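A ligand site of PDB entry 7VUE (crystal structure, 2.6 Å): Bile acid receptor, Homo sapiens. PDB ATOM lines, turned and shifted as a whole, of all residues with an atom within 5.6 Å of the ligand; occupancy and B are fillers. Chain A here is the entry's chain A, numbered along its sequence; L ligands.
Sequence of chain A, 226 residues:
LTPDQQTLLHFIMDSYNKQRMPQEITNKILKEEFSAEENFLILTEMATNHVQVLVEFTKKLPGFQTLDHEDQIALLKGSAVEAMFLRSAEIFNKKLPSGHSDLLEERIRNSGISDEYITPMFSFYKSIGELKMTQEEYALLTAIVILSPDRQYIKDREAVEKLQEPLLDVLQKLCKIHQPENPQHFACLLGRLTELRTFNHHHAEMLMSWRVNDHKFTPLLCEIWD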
ATOM      1  N   ARG A  20       5.331   7.513  15.051  1.00  0.00           N
ATOM      2  CA  ARG A  20       6.261   6.993  14.074  1.00  0.00           C
ATOM      3  C   ARG A  20       5.970   7.675  12.747  1.00  0.00           C
ATOM      4  O   ARG A  20       5.116   8.572  12.679  1.00  0.00           O
ATOM      5  CB  ARG A  20       6.158   5.474  13.943  1.00  0.00           C
ATOM      6  N   MET A  21       6.672   7.279  11.700  1.00  0.00           N
ATOM      7  CA  MET A  21       6.418   7.879  10.396  1.00  0.00           C
ATOM      8  C   MET A  21       5.206   7.215   9.748  1.00  0.00           C
ATOM      9  O   MET A  21       5.149   5.988   9.642  1.00  0.00           O
ATOM     10  CB  MET A  21       7.634   7.756   9.489  1.00  0.00           C
ATOM     11  CG  MET A  21       7.552   8.655   8.272  1.00  0.00           C
ATOM     12  SD  MET A  21       8.734  10.013   8.382  1.00  0.00           S
ATOM     13  CE  MET A  21      10.198   9.151   7.892  1.00  0.00           C
ATOM     14  N   THR A  26       6.215   6.222   4.535  1.00  0.00           N
ATOM     15  CA  THR A  26       7.271   5.213   4.566  1.00  0.00           C
ATOM     16  C   THR A  26       7.090   4.094   3.533  1.00  0.00           C
ATOM     17  O   THR A  26       8.056   3.421   3.186  1.00  0.00           O
ATOM     18  CB  THR A  26       7.428   4.561   5.969  1.00  0.00           C
ATOM     19  OG1 THR A  26       6.145   4.361   6.565  1.00  0.00           O
ATOM     20  CG2 THR A  26       8.266   5.428   6.882  1.00  0.00           C
ATOM     21  N   PHE A  40      15.273  11.968  -3.693  1.00  0.00           N
ATOM     22  CA  PHE A  40      15.376  13.183  -2.916  1.00  0.00           C
ATOM     23  C   PHE A  40      14.021  13.622  -2.374  1.00  0.00           C
ATOM     24  O   PHE A  40      13.934  14.150  -1.260  1.00  0.00           O
ATOM     25  CB  PHE A  40      16.008  14.286  -3.759  1.00  0.00           C
ATOM     26  CG  PHE A  40      16.293  15.514  -2.971  1.00  0.00           C
ATOM     27  CD1 PHE A  40      17.427  15.586  -2.188  1.00  0.00           C
ATOM     28  CD2 PHE A  40      15.430  16.589  -3.004  1.00  0.00           C
ATOM     29  CE1 PHE A  40      17.691  16.721  -1.447  1.00  0.00           C
ATOM     30  CE2 PHE A  40      15.686  17.720  -2.276  1.00  0.00           C
ATOM     31  CZ  PHE A  40      16.822  17.783  -1.491  1.00  0.00           C
ATOM     32  N   ILE A  42      11.388  11.752  -1.495  1.00  0.00           N
ATOM     33  CA  ILE A  42      10.975  10.930  -0.382  1.00  0.00           C
ATOM     34  C   ILE A  42      11.761  11.308   0.866  1.00  0.00           C
ATOM     35  O   ILE A  42      11.182  11.447   1.945  1.00  0.00           O
ATOM     36  CB  ILE A  42      11.173   9.440  -0.687  1.00  0.00           C
ATOM     37  CG1 ILE A  42      10.276   9.045  -1.862  1.00  0.00           C
ATOM     38  CG2 ILE A  42      10.876   8.587   0.540  1.00  0.00           C
ATOM     39  CD1 ILE A  42      10.487   7.650  -2.345  1.00  0.00           C
ATOM     40  N   LEU A  43      13.065  11.483   0.714  1.00  0.00           N
ATOM     41  CA  LEU A  43      13.916  11.899   1.808  1.00  0.00           C
ATOM     42  C   LEU A  43      13.415  13.218   2.399  1.00  0.00           C
ATOM     43  O   LEU A  43      13.409  13.405   3.616  1.00  0.00           O
ATOM     44  CB  LEU A  43      15.361  12.040   1.347  1.00  0.00           C
ATOM     45  CG  LEU A  43      16.055  10.730   0.972  1.00  0.00           C
ATOM     46  CD1 LEU A  43      17.410  11.019   0.372  1.00  0.00           C
ATOM     47  CD2 LEU A  43      16.198   9.835   2.189  1.00  0.00           C
ATOM     48  N   THR A  44      12.998  14.121   1.521  1.00  0.00           N
ATOM     49  CA  THR A  44      12.413  15.388   1.939  1.00  0.00           C
ATOM     50  C   THR A  44      11.098  15.137   2.686  1.00  0.00           C
ATOM     51  O   THR A  44      10.901  15.649   3.792  1.00  0.00           O
ATOM     52  CB  THR A  44      12.153  16.320   0.740  1.00  0.00           C
ATOM     53  OG1 THR A  44      13.388  16.559   0.051  1.00  0.00           O
ATOM     54  CG2 THR A  44      11.576  17.638   1.216  1.00  0.00           C
ATOM     55  N   MET A  46      10.244  12.737   4.265  1.00  0.00           N
ATOM     56  CA  MET A  46      10.522  12.008   5.481  1.00  0.00           C
ATOM     57  C   MET A  46      11.229  12.851   6.536  1.00  0.00           C
ATOM     58  O   MET A  46      10.993  12.681   7.731  1.00  0.00           O
ATOM     59  CB  MET A  46      11.346  10.777   5.153  1.00  0.00           C
ATOM     60  CG  MET A  46      10.609   9.662   4.471  1.00  0.00           C
ATOM     61  SD  MET A  46      11.657   8.212   4.465  1.00  0.00           S
ATOM     62  CE  MET A  46      13.049   8.866   3.567  1.00  0.00           C
ATOM     63  N   ALA A  47      12.106  13.738   6.090  1.00  0.00           N
ATOM     64  CA  ALA A  47      12.827  14.617   6.992  1.00  0.00           C
ATOM     65  C   ALA A  47      11.888  15.699   7.505  1.00  0.00           C
ATOM     66  O   ALA A  47      11.942  16.090   8.664  1.00  0.00           O
ATOM     67  CB  ALA A  47      14.029  15.232   6.308  1.00  0.00           C
ATOM     68  N   THR A  48      11.026  16.185   6.612  1.00  0.00           N
ATOM     69  CA  THR A  48      10.012  17.159   6.978  1.00  0.00           C
ATOM     70  C   THR A  48       9.052  16.555   7.968  1.00  0.00           C
ATOM     71  O   THR A  48       8.735  17.174   8.994  1.00  0.00           O
ATOM     72  CB  THR A  48       9.204  17.628   5.761  1.00  0.00           C
ATOM     73  OG1 THR A  48      10.109  18.092   4.752  1.00  0.00           O
ATOM     74  CG2 THR A  48       8.263  18.747   6.158  1.00  0.00           C
ATOM     75  N   HIS A  50       9.686  14.149   9.849  1.00  0.00           N
ATOM     76  CA  HIS A  50      10.430  13.892  11.059  1.00  0.00           C
ATOM     77  C   HIS A  50      10.637  15.157  11.881  1.00  0.00           C
ATOM     78  O   HIS A  50      10.801  15.085  13.097  1.00  0.00           O
ATOM     79  CB  HIS A  50      11.775  13.238  10.726  1.00  0.00           C
ATOM     80  CG  HIS A  50      12.398  12.543  11.888  1.00  0.00           C
ATOM     81  ND1 HIS A  50      13.552  13.003  12.502  1.00  0.00           N
ATOM     82  CD2 HIS A  50      12.029  11.442  12.573  1.00  0.00           C
ATOM     83  CE1 HIS A  50      13.861  12.204  13.506  1.00  0.00           C
ATOM     84  NE2 HIS A  50      12.959  11.243  13.566  1.00  0.00           N
ATOM     85  N   VAL A  81      19.024  18.202  12.488  1.00  0.00           N
ATOM     86  CA  VAL A  81      19.865  17.387  11.631  1.00  0.00           C
ATOM     87  C   VAL A  81      20.359  16.129  12.327  1.00  0.00           C
ATOM     88  O   VAL A  81      20.198  15.017  11.827  1.00  0.00           O
ATOM     89  CB  VAL A  81      21.095  18.169  11.163  1.00  0.00           C
ATOM     90  CG1 VAL A  81      21.976  17.297  10.277  1.00  0.00           C
ATOM     91  CG2 VAL A  81      20.673  19.442  10.448  1.00  0.00           C
ATOM     92  N   MET A  84      17.621  13.669  13.498  1.00  0.00           N
ATOM     93  CA  MET A  84      17.200  12.863  12.358  1.00  0.00           C
ATOM     94  C   MET A  84      18.131  11.669  12.219  1.00  0.00           C
ATOM     95  O   MET A  84      17.687  10.529  12.039  1.00  0.00           O
ATOM     96  CB  MET A  84      17.217  13.672  11.055  1.00  0.00           C
ATOM     97  CG  MET A  84      16.146  14.742  10.955  1.00  0.00           C
ATOM     98  SD  MET A  84      16.215  15.568   9.353  1.00  0.00           S
ATOM     99  CE  MET A  84      15.037  16.883   9.612  1.00  0.00           C
ATOM    100  N   PHE A  85      19.422  11.954  12.311  1.00  0.00           N
ATOM    101  CA  PHE A  85      20.461  10.951  12.166  1.00  0.00           C
ATOM    102  C   PHE A  85      20.304   9.813  13.165  1.00  0.00           C
ATOM    103  O   PHE A  85      20.408   8.636  12.809  1.00  0.00           O
ATOM    104  CB  PHE A  85      21.824  11.603  12.332  1.00  0.00           C
ATOM    105  CG  PHE A  85      22.930  10.888  11.626  1.00  0.00           C
ATOM    106  CD1 PHE A  85      23.481  11.396  10.470  1.00  0.00           C
ATOM    107  CD2 PHE A  85      23.392   9.680  12.108  1.00  0.00           C
ATOM    108  CE1 PHE A  85      24.503  10.730   9.816  1.00  0.00           C
ATOM    109  CE2 PHE A  85      24.407   9.002  11.454  1.00  0.00           C
ATOM    110  CZ  PHE A  85      24.961   9.532  10.308  1.00  0.00           C
ATOM    111  N   ARG A  87      17.629   8.799  14.783  1.00  0.00           N
ATOM    112  CA  ARG A  87      16.397   8.043  14.617  1.00  0.00           C
ATOM    113  C   ARG A  87      16.446   7.121  13.396  1.00  0.00           C
ATOM    114  O   ARG A  87      15.707   6.140  13.313  1.00  0.00           O
ATOM    115  CB  ARG A  87      15.214   9.015  14.526  1.00  0.00           C
ATOM    116  CG  ARG A  87      13.847   8.385  14.550  1.00  0.00           C
ATOM    117  CD  ARG A  87      13.617   7.469  15.723  1.00  0.00           C
ATOM    118  NE  ARG A  87      12.213   7.066  15.815  1.00  0.00           N
ATOM    119  CZ  ARG A  87      11.733   5.906  15.365  1.00  0.00           C
ATOM    120  NH1 ARG A  87      12.555   5.028  14.805  1.00  0.00           N
ATOM    121  NH2 ARG A  87      10.440   5.625  15.486  1.00  0.00           N
ATOM    122  N   SER A  88      17.342   7.414  12.450  1.00  0.00           N
ATOM    123  CA  SER A  88      17.522   6.560  11.277  1.00  0.00           C
ATOM    124  C   SER A  88      18.588   5.506  11.517  1.00  0.00           C
ATOM    125  O   SER A  88      18.546   4.423  10.944  1.00  0.00           O
ATOM    126  CB  SER A  88      17.885   7.397  10.051  1.00  0.00           C
ATOM    127  OG  SER A  88      19.165   7.985  10.188  1.00  0.00           O
ATOM    128  N   ILE A  91      16.780   3.005  13.018  1.00  0.00           N
ATOM    129  CA  ILE A  91      16.099   2.330  11.924  1.00  0.00           C
ATOM    130  C   ILE A  91      16.997   1.328  11.213  1.00  0.00           C
ATOM    131  O   ILE A  91      16.576   0.219  10.902  1.00  0.00           O
ATOM    132  CB  ILE A  91      15.571   3.353  10.894  1.00  0.00           C
ATOM    133  CG1 ILE A  91      14.282   4.001  11.411  1.00  0.00           C
ATOM    134  CG2 ILE A  91      15.302   2.683   9.556  1.00  0.00           C
ATOM    135  CD1 ILE A  91      13.234   3.011  11.856  1.00  0.00           C
ATOM    136  N   SER A  98       9.684  -0.999   9.231  1.00  0.00           N
ATOM    137  CA  SER A  98       8.868   0.148   8.843  1.00  0.00           C
ATOM    138  C   SER A  98       9.737   1.242   8.237  1.00  0.00           C
ATOM    139  O   SER A  98       9.233   2.213   7.674  1.00  0.00           O
ATOM    140  CB  SER A  98       8.086   0.687  10.038  1.00  0.00           C
ATOM    141  N   GLY A  99      11.050   1.091   8.367  1.00  0.00           N
ATOM    142  CA  GLY A  99      11.993   2.056   7.834  1.00  0.00           C
ATOM    143  C   GLY A  99      12.634   1.596   6.537  1.00  0.00           C
ATOM    144  O   GLY A  99      13.228   2.405   5.823  1.00  0.00           O
ATOM    145  N   LEU A 104      16.271   2.257   1.918  1.00  0.00           N
ATOM    146  CA  LEU A 104      16.409   3.642   2.321  1.00  0.00           C
ATOM    147  C   LEU A 104      17.833   4.111   2.055  1.00  0.00           C
ATOM    148  O   LEU A 104      18.055   5.252   1.647  1.00  0.00           O
ATOM    149  CB  LEU A 104      16.040   3.826   3.790  1.00  0.00           C
ATOM    150  CG  LEU A 104      16.082   5.257   4.335  1.00  0.00           C
ATOM    151  CD1 LEU A 104      15.384   6.198   3.384  1.00  0.00           C
ATOM    152  CD2 LEU A 104      15.471   5.333   5.729  1.00  0.00           C
ATOM    153  N   ILE A 108      19.317   7.267  -0.584  1.00  0.00           N
ATOM    154  CA  ILE A 108      20.217   8.296  -0.070  1.00  0.00           C
ATOM    155  C   ILE A 108      21.493   8.433  -0.916  1.00  0.00           C
ATOM    156  O   ILE A 108      21.947   9.553  -1.180  1.00  0.00           O
ATOM    157  CB  ILE A 108      20.597   7.995   1.406  1.00  0.00           C
ATOM    158  CG1 ILE A 108      19.343   8.043   2.282  1.00  0.00           C
ATOM    159  CG2 ILE A 108      21.637   8.974   1.907  1.00  0.00           C
ATOM    160  CD1 ILE A 108      19.602   7.733   3.747  1.00  0.00           C
ATOM    161  N   ILE A 113      23.913  13.552  -3.261  1.00  0.00           N
ATOM    162  CA  ILE A 113      24.875  13.753  -2.192  1.00  0.00           C
ATOM    163  C   ILE A 113      26.254  13.347  -2.682  1.00  0.00           C
ATOM    164  O   ILE A 113      26.432  12.255  -3.246  1.00  0.00           O
ATOM    165  CB  ILE A 113      24.541  12.938  -0.923  1.00  0.00           C
ATOM    166  CG1 ILE A 113      23.079  13.092  -0.560  1.00  0.00           C
ATOM    167  CG2 ILE A 113      25.431  13.371   0.237  1.00  0.00           C
ATOM    168  CD1 ILE A 113      22.644  12.193   0.555  1.00  0.00           C
ATOM    169  N   MET A 121      29.000   9.011   6.586  1.00  0.00           N
ATOM    170  CA  MET A 121      27.653   8.909   7.092  1.00  0.00           C
ATOM    171  C   MET A 121      27.268   7.466   7.373  1.00  0.00           C
ATOM    172  O   MET A 121      26.557   7.167   8.342  1.00  0.00           O
ATOM    173  CB  MET A 121      26.704   9.558   6.090  1.00  0.00           C
ATOM    174  CG  MET A 121      25.242   9.344   6.319  1.00  0.00           C
ATOM    175  SD  MET A 121      24.406   9.887   4.825  1.00  0.00           S
ATOM    176  CE  MET A 121      25.200  11.456   4.534  1.00  0.00           C
ATOM    177  N   TYR A 125      26.635   5.050  10.438  1.00  0.00           N
ATOM    178  CA  TYR A 125      25.434   4.214  10.406  1.00  0.00           C
ATOM    179  C   TYR A 125      25.710   2.804  10.872  1.00  0.00           C
ATOM    180  O   TYR A 125      24.955   2.224  11.651  1.00  0.00           O
ATOM    181  CB  TYR A 125      24.843   4.194   9.001  1.00  0.00           C
ATOM    182  CG  TYR A 125      23.812   5.260   8.786  1.00  0.00           C
ATOM    183  CD1 TYR A 125      23.349   6.014   9.857  1.00  0.00           C
ATOM    184  CD2 TYR A 125      23.306   5.516   7.526  1.00  0.00           C
ATOM    185  CE1 TYR A 125      22.399   6.998   9.663  1.00  0.00           C
ATOM    186  CE2 TYR A 125      22.355   6.499   7.332  1.00  0.00           C
ATOM    187  CZ  TYR A 125      21.906   7.237   8.407  1.00  0.00           C
ATOM    188  OH  TYR A 125      20.960   8.210   8.204  1.00  0.00           O
ATOM    189  N   PHE A 199      29.119  15.771  11.610  1.00  0.00           N
ATOM    190  CA  PHE A 199      28.201  15.585  10.496  1.00  0.00           C
ATOM    191  C   PHE A 199      27.341  16.821  10.247  1.00  0.00           C
ATOM    192  O   PHE A 199      26.965  17.102   9.110  1.00  0.00           O
ATOM    193  CB  PHE A 199      27.304  14.377  10.730  1.00  0.00           C
ATOM    194  CG  PHE A 199      26.326  14.137   9.621  1.00  0.00           C
ATOM    195  CD1 PHE A 199      26.748  13.684   8.386  1.00  0.00           C
ATOM    196  CD2 PHE A 199      24.978  14.400   9.811  1.00  0.00           C
ATOM    197  CE1 PHE A 199      25.852  13.483   7.359  1.00  0.00           C
ATOM    198  CE2 PHE A 199      24.070  14.207   8.782  1.00  0.00           C
ATOM    199  CZ  PHE A 199      24.503  13.746   7.550  1.00  0.00           C
ATOM    200  N   HIS A 203      26.767  18.417   6.679  1.00  0.00           N
ATOM    201  CA  HIS A 203      25.404  18.468   6.171  1.00  0.00           C
ATOM    202  C   HIS A 203      25.051  19.820   5.554  1.00  0.00           C
ATOM    203  O   HIS A 203      24.396  19.871   4.508  1.00  0.00           O
ATOM    204  CB  HIS A 203      24.404  18.158   7.273  1.00  0.00           C
ATOM    205  CG  HIS A 203      22.977  18.222   6.814  1.00  0.00           C
ATOM    206  ND1 HIS A 203      22.003  18.940   7.472  1.00  0.00           N
ATOM    207  CD2 HIS A 203      22.361  17.647   5.744  1.00  0.00           C
ATOM    208  CE1 HIS A 203      20.851  18.810   6.843  1.00  0.00           C
ATOM    209  NE2 HIS A 203      21.045  18.035   5.788  1.00  0.00           N
ATOM    210  N   MET A 206      26.029  19.657   2.205  1.00  0.00           N
ATOM    211  CA  MET A 206      25.145  18.824   1.403  1.00  0.00           C
ATOM    212  C   MET A 206      23.945  19.649   0.985  1.00  0.00           C
ATOM    213  O   MET A 206      23.416  19.493  -0.124  1.00  0.00           O
ATOM    214  CB  MET A 206      24.655  17.612   2.177  1.00  0.00           C
ATOM    215  CG  MET A 206      25.727  16.711   2.732  1.00  0.00           C
ATOM    216  SD  MET A 206      24.991  15.515   3.859  1.00  0.00           S
ATOM    217  CE  MET A 206      23.535  15.030   2.940  1.00  0.00           C
ATOM    218  N   LEU A 207      23.510  20.515   1.898  1.00  0.00           N
ATOM    219  CA  LEU A 207      22.362  21.387   1.679  1.00  0.00           C
ATOM    220  C   LEU A 207      22.611  22.341   0.526  1.00  0.00           C
ATOM    221  O   LEU A 207      21.746  22.530  -0.333  1.00  0.00           O
ATOM    222  CB  LEU A 207      22.038  22.177   2.944  1.00  0.00           C
ATOM    223  CG  LEU A 207      21.494  21.351   4.106  1.00  0.00           C
ATOM    224  CD1 LEU A 207      21.063  22.275   5.230  1.00  0.00           C
ATOM    225  CD2 LEU A 207      20.347  20.477   3.648  1.00  0.00           C
ATOM    226  N   TRP A 210      22.874  20.725  -2.823  1.00  0.00           N
ATOM    227  CA  TRP A 210      21.510  20.503  -3.288  1.00  0.00           C
ATOM    228  C   TRP A 210      20.871  21.778  -3.818  1.00  0.00           C
ATOM    229  O   TRP A 210      20.402  21.818  -4.962  1.00  0.00           O
ATOM    230  CB  TRP A 210      20.671  19.914  -2.157  1.00  0.00           C
ATOM    231  CG  TRP A 210      20.840  18.427  -1.948  1.00  0.00           C
ATOM    232  CD1 TRP A 210      21.132  17.500  -2.912  1.00  0.00           C
ATOM    233  CD2 TRP A 210      20.727  17.711  -0.719  1.00  0.00           C
ATOM    234  NE1 TRP A 210      21.185  16.247  -2.345  1.00  0.00           N
ATOM    235  CE2 TRP A 210      20.948  16.355  -0.990  1.00  0.00           C
ATOM    236  CE3 TRP A 210      20.447  18.085   0.608  1.00  0.00           C
ATOM    237  CZ2 TRP A 210      20.902  15.365  -0.013  1.00  0.00           C
ATOM    238  CZ3 TRP A 210      20.409  17.108   1.585  1.00  0.00           C
ATOM    239  CH2 TRP A 210      20.633  15.766   1.263  1.00  0.00           C
ATOM    240  N   PHE A 217      13.250  22.335  -0.941  1.00  0.00           N
ATOM    241  CA  PHE A 217      12.782  21.799   0.333  1.00  0.00           C
ATOM    242  C   PHE A 217      11.430  22.365   0.723  1.00  0.00           C
ATOM    243  O   PHE A 217      10.867  23.202   0.018  1.00  0.00           O
ATOM    244  CB  PHE A 217      13.791  22.119   1.442  1.00  0.00           C
ATOM    245  CG  PHE A 217      15.185  21.734   1.095  1.00  0.00           C
ATOM    246  CD1 PHE A 217      16.047  22.641   0.502  1.00  0.00           C
ATOM    247  CD2 PHE A 217      15.645  20.458   1.369  1.00  0.00           C
ATOM    248  CE1 PHE A 217      17.337  22.285   0.176  1.00  0.00           C
ATOM    249  CE2 PHE A 217      16.934  20.093   1.054  1.00  0.00           C
ATOM    250  CZ  PHE A 217      17.785  21.008   0.458  1.00  0.00           C
ATOM    251  N   LEU A 221      11.552  22.877   6.427  1.00  0.00           N
ATOM    252  CA  LEU A 221      12.979  22.580   6.324  1.00  0.00           C
ATOM    253  C   LEU A 221      13.776  23.828   5.937  1.00  0.00           C
ATOM    254  O   LEU A 221      14.863  24.043   6.446  1.00  0.00           O
ATOM    255  CB  LEU A 221      13.222  21.469   5.304  1.00  0.00           C
ATOM    256  CG  LEU A 221      12.759  20.062   5.691  1.00  0.00           C
ATOM    257  CD1 LEU A 221      13.170  19.057   4.621  1.00  0.00           C
ATOM    258  CD2 LEU A 221      13.305  19.672   7.050  1.00  0.00           C
ATOM    259  N   TRP A 225      16.586  25.366   8.639  1.00  0.00           N
ATOM    260  CA  TRP A 225      17.946  25.385   8.112  1.00  0.00           C
ATOM    261  C   TRP A 225      18.230  26.687   7.376  1.00  0.00           C
ATOM    262  O   TRP A 225      19.292  26.855   6.775  1.00  0.00           O
ATOM    263  CB  TRP A 225      18.168  24.177   7.188  1.00  0.00           C
ATOM    264  CG  TRP A 225      18.077  22.843   7.879  1.00  0.00           C
ATOM    265  CD1 TRP A 225      18.334  22.587   9.197  1.00  0.00           C
ATOM    266  CD2 TRP A 225      17.702  21.597   7.291  1.00  0.00           C
ATOM    267  NE1 TRP A 225      18.143  21.250   9.463  1.00  0.00           N
ATOM    268  CE2 TRP A 225      17.754  20.615   8.305  1.00  0.00           C
ATOM    269  CE3 TRP A 225      17.327  21.197   5.995  1.00  0.00           C
ATOM    270  CZ2 TRP A 225      17.443  19.272   8.072  1.00  0.00           C
ATOM    271  CZ3 TRP A 225      17.020  19.876   5.771  1.00  0.00           C
ATOM    272  CH2 TRP A 225      17.080  18.929   6.804  1.00  0.00           C
HETATM  273  O1  LIG L   1       8.622   4.981  11.308  1.00  0.00           O
HETATM  274  C1  LIG L   1       9.633   4.911  10.554  1.00  0.00           C
HETATM  275  O2  LIG L   1       9.661   4.069   9.608  1.00  0.00           O
HETATM  276  C2  LIG L   1      10.813   5.838  10.779  1.00  0.00           C
HETATM  277  C3  LIG L   1      11.268   6.713   9.771  1.00  0.00           C
HETATM  278  C4  LIG L   1      11.501   5.869  12.007  1.00  0.00           C
HETATM  279  C5  LIG L   1      12.572   6.731  12.167  1.00  0.00           C
HETATM  280  N1  LIG L   1      12.969   7.533  11.185  1.00  0.00           N
HETATM  281  C6  LIG L   1      12.356   7.537  10.018  1.00  0.00           C
HETATM  282  N2  LIG L   1      12.821   8.432   8.980  1.00  0.00           N
HETATM  283  C7  LIG L   1      14.229   8.160   8.688  1.00  0.00           C
HETATM  284  C8  LIG L   1      13.184   9.717   9.572  1.00  0.00           C
HETATM  285  C9  LIG L   1      14.567   9.523   9.117  1.00  0.00           C
HETATM  286  O3  LIG L   1      15.500   9.551  10.185  1.00  0.00           O
HETATM  287  C10 LIG L   1      14.931  10.432   7.968  1.00  0.00           C
HETATM  288  C11 LIG L   1      16.232  10.898   7.833  1.00  0.00           C
HETATM  289 CL1  LIG L   1      17.451  10.437   9.000  1.00  0.00          CL
HETATM  290  C12 LIG L   1      16.577  11.742   6.778  1.00  0.00           C
HETATM  291  C13 LIG L   1      13.968  10.806   7.037  1.00  0.00           C
HETATM  292  C14 LIG L   1      14.306  11.637   5.981  1.00  0.00           C
HETATM  293  C15 LIG L   1      15.605  12.104   5.856  1.00  0.00           C
HETATM  294  O4  LIG L   1      15.951  12.965   4.768  1.00  0.00           O
HETATM  295  C16 LIG L   1      17.262  12.758   4.261  1.00  0.00           C
HETATM  296  C17 LIG L   1      18.096  14.023   4.541  1.00  0.00           C
HETATM  297  C18 LIG L   1      17.799  15.376   4.167  1.00  0.00           C
HETATM  298  C19 LIG L   1      16.576  15.853   3.396  1.00  0.00           C
HETATM  299  C20 LIG L   1      15.357  16.515   3.374  1.00  0.00           C
HETATM  300  C21 LIG L   1      15.862  15.935   2.215  1.00  0.00           C
HETATM  301  O5  LIG L   1      18.787  16.140   4.616  1.00  0.00           O
HETATM  302  N3  LIG L   1      19.691  15.404   5.240  1.00  0.00           N
HETATM  303  C22 LIG L   1      19.350  14.124   5.242  1.00  0.00           C
HETATM  304  C23 LIG L   1      20.141  12.969   5.869  1.00  0.00           C
HETATM  305  C24 LIG L   1      20.720  12.013   5.049  1.00  0.00           C
HETATM  306 CL2  LIG L   1      20.557  12.116   3.311  1.00  0.00          CL
HETATM  307  C25 LIG L   1      21.443  10.959   5.616  1.00  0.00           C
HETATM  308  C26 LIG L   1      21.573  10.878   7.000  1.00  0.00           C
HETATM  309  C27 LIG L   1      20.993  11.842   7.809  1.00  0.00           C
HETATM  310  C28 LIG L   1      20.272  12.887   7.243  1.00  0.00           C
HETATM  311 CL3  LIG L   1      19.543  14.101   8.271  1.00  0.00          CL
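OH of Tyr 125 is in hydrogen-bond range of OG of Ser 88 (2.7 Å). O of Met 84 sits at hydrogen-bond distance from OG of Ser 88, at 3.5 Å. The side-chain hydroxyl (OG) of Ser 88 is in hydrogen-bond range of the backbone carbonyl oxygen (O) of Phe 85, at 3.0 Å. The side-chain hydroxyl of Thr 44 is in hydrogen-bond range of the backbone carbonyl oxygen of Phe 40. The backbone carbonyl oxygen (O) of Thr 44 lies within hydrogen-bond range of the side-chain hydroxyl (OG1) of Thr 48, at 2.7 Å.
O of Ser 98 lies close to O2 of the ligand, 2.7 Å away. An oxygen (O1) of the ligand is in hydrogen-bond range of the backbone NH (N) of Met 21 (3.0 Å). NE2 of His 203 is in hydrogen-bond range of N3 of the ligand, 3.0 Å away. The backbone carbonyl oxygen (O) of Met 84 is in hydrogen-bond range of an oxygen (O3) of the ligand (3.0 Å).
An oxygen (O4) of the ligand lies close to the backbone carbonyl oxygen of Leu 43 (2.8 Å). Residues that only touch the ligand: Tyr 125 (3.0 Å), Ala 47 (3.0 Å), Arg 87 (3.1 Å), Met 46 (3.2 Å), Ser 88 (3.2 Å), Met 121 (3.2 Å), Ile 91 (3.3 Å), Thr 44 (3.3 Å), Thr 26 (3.4 Å), Ile 113 (3.5 Å), Gly 99 (3.5 Å), Trp 210 (3.6 Å), Leu 221 (3.6 Å), Ile 108 (3.6 Å), Arg 20 (3.6 Å), His 50 (3.6 Å), Phe 85 (3.7 Å), Val 81 (3.7 Å) and Trp 225 (3.9 Å). Hydrophobic or aromatic side chains within 4 Å of the ligand: Met 21, Leu 43, Met 46, Ala 47, His 50, Met 84, Phe 85, Ile 91, Ile 108, Ile 113, Met 121, Tyr 125, His 203, Trp 210, Leu 221 and Trp 225. Of the 32 residues printed, 24 come within 4 Å of the ligand.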
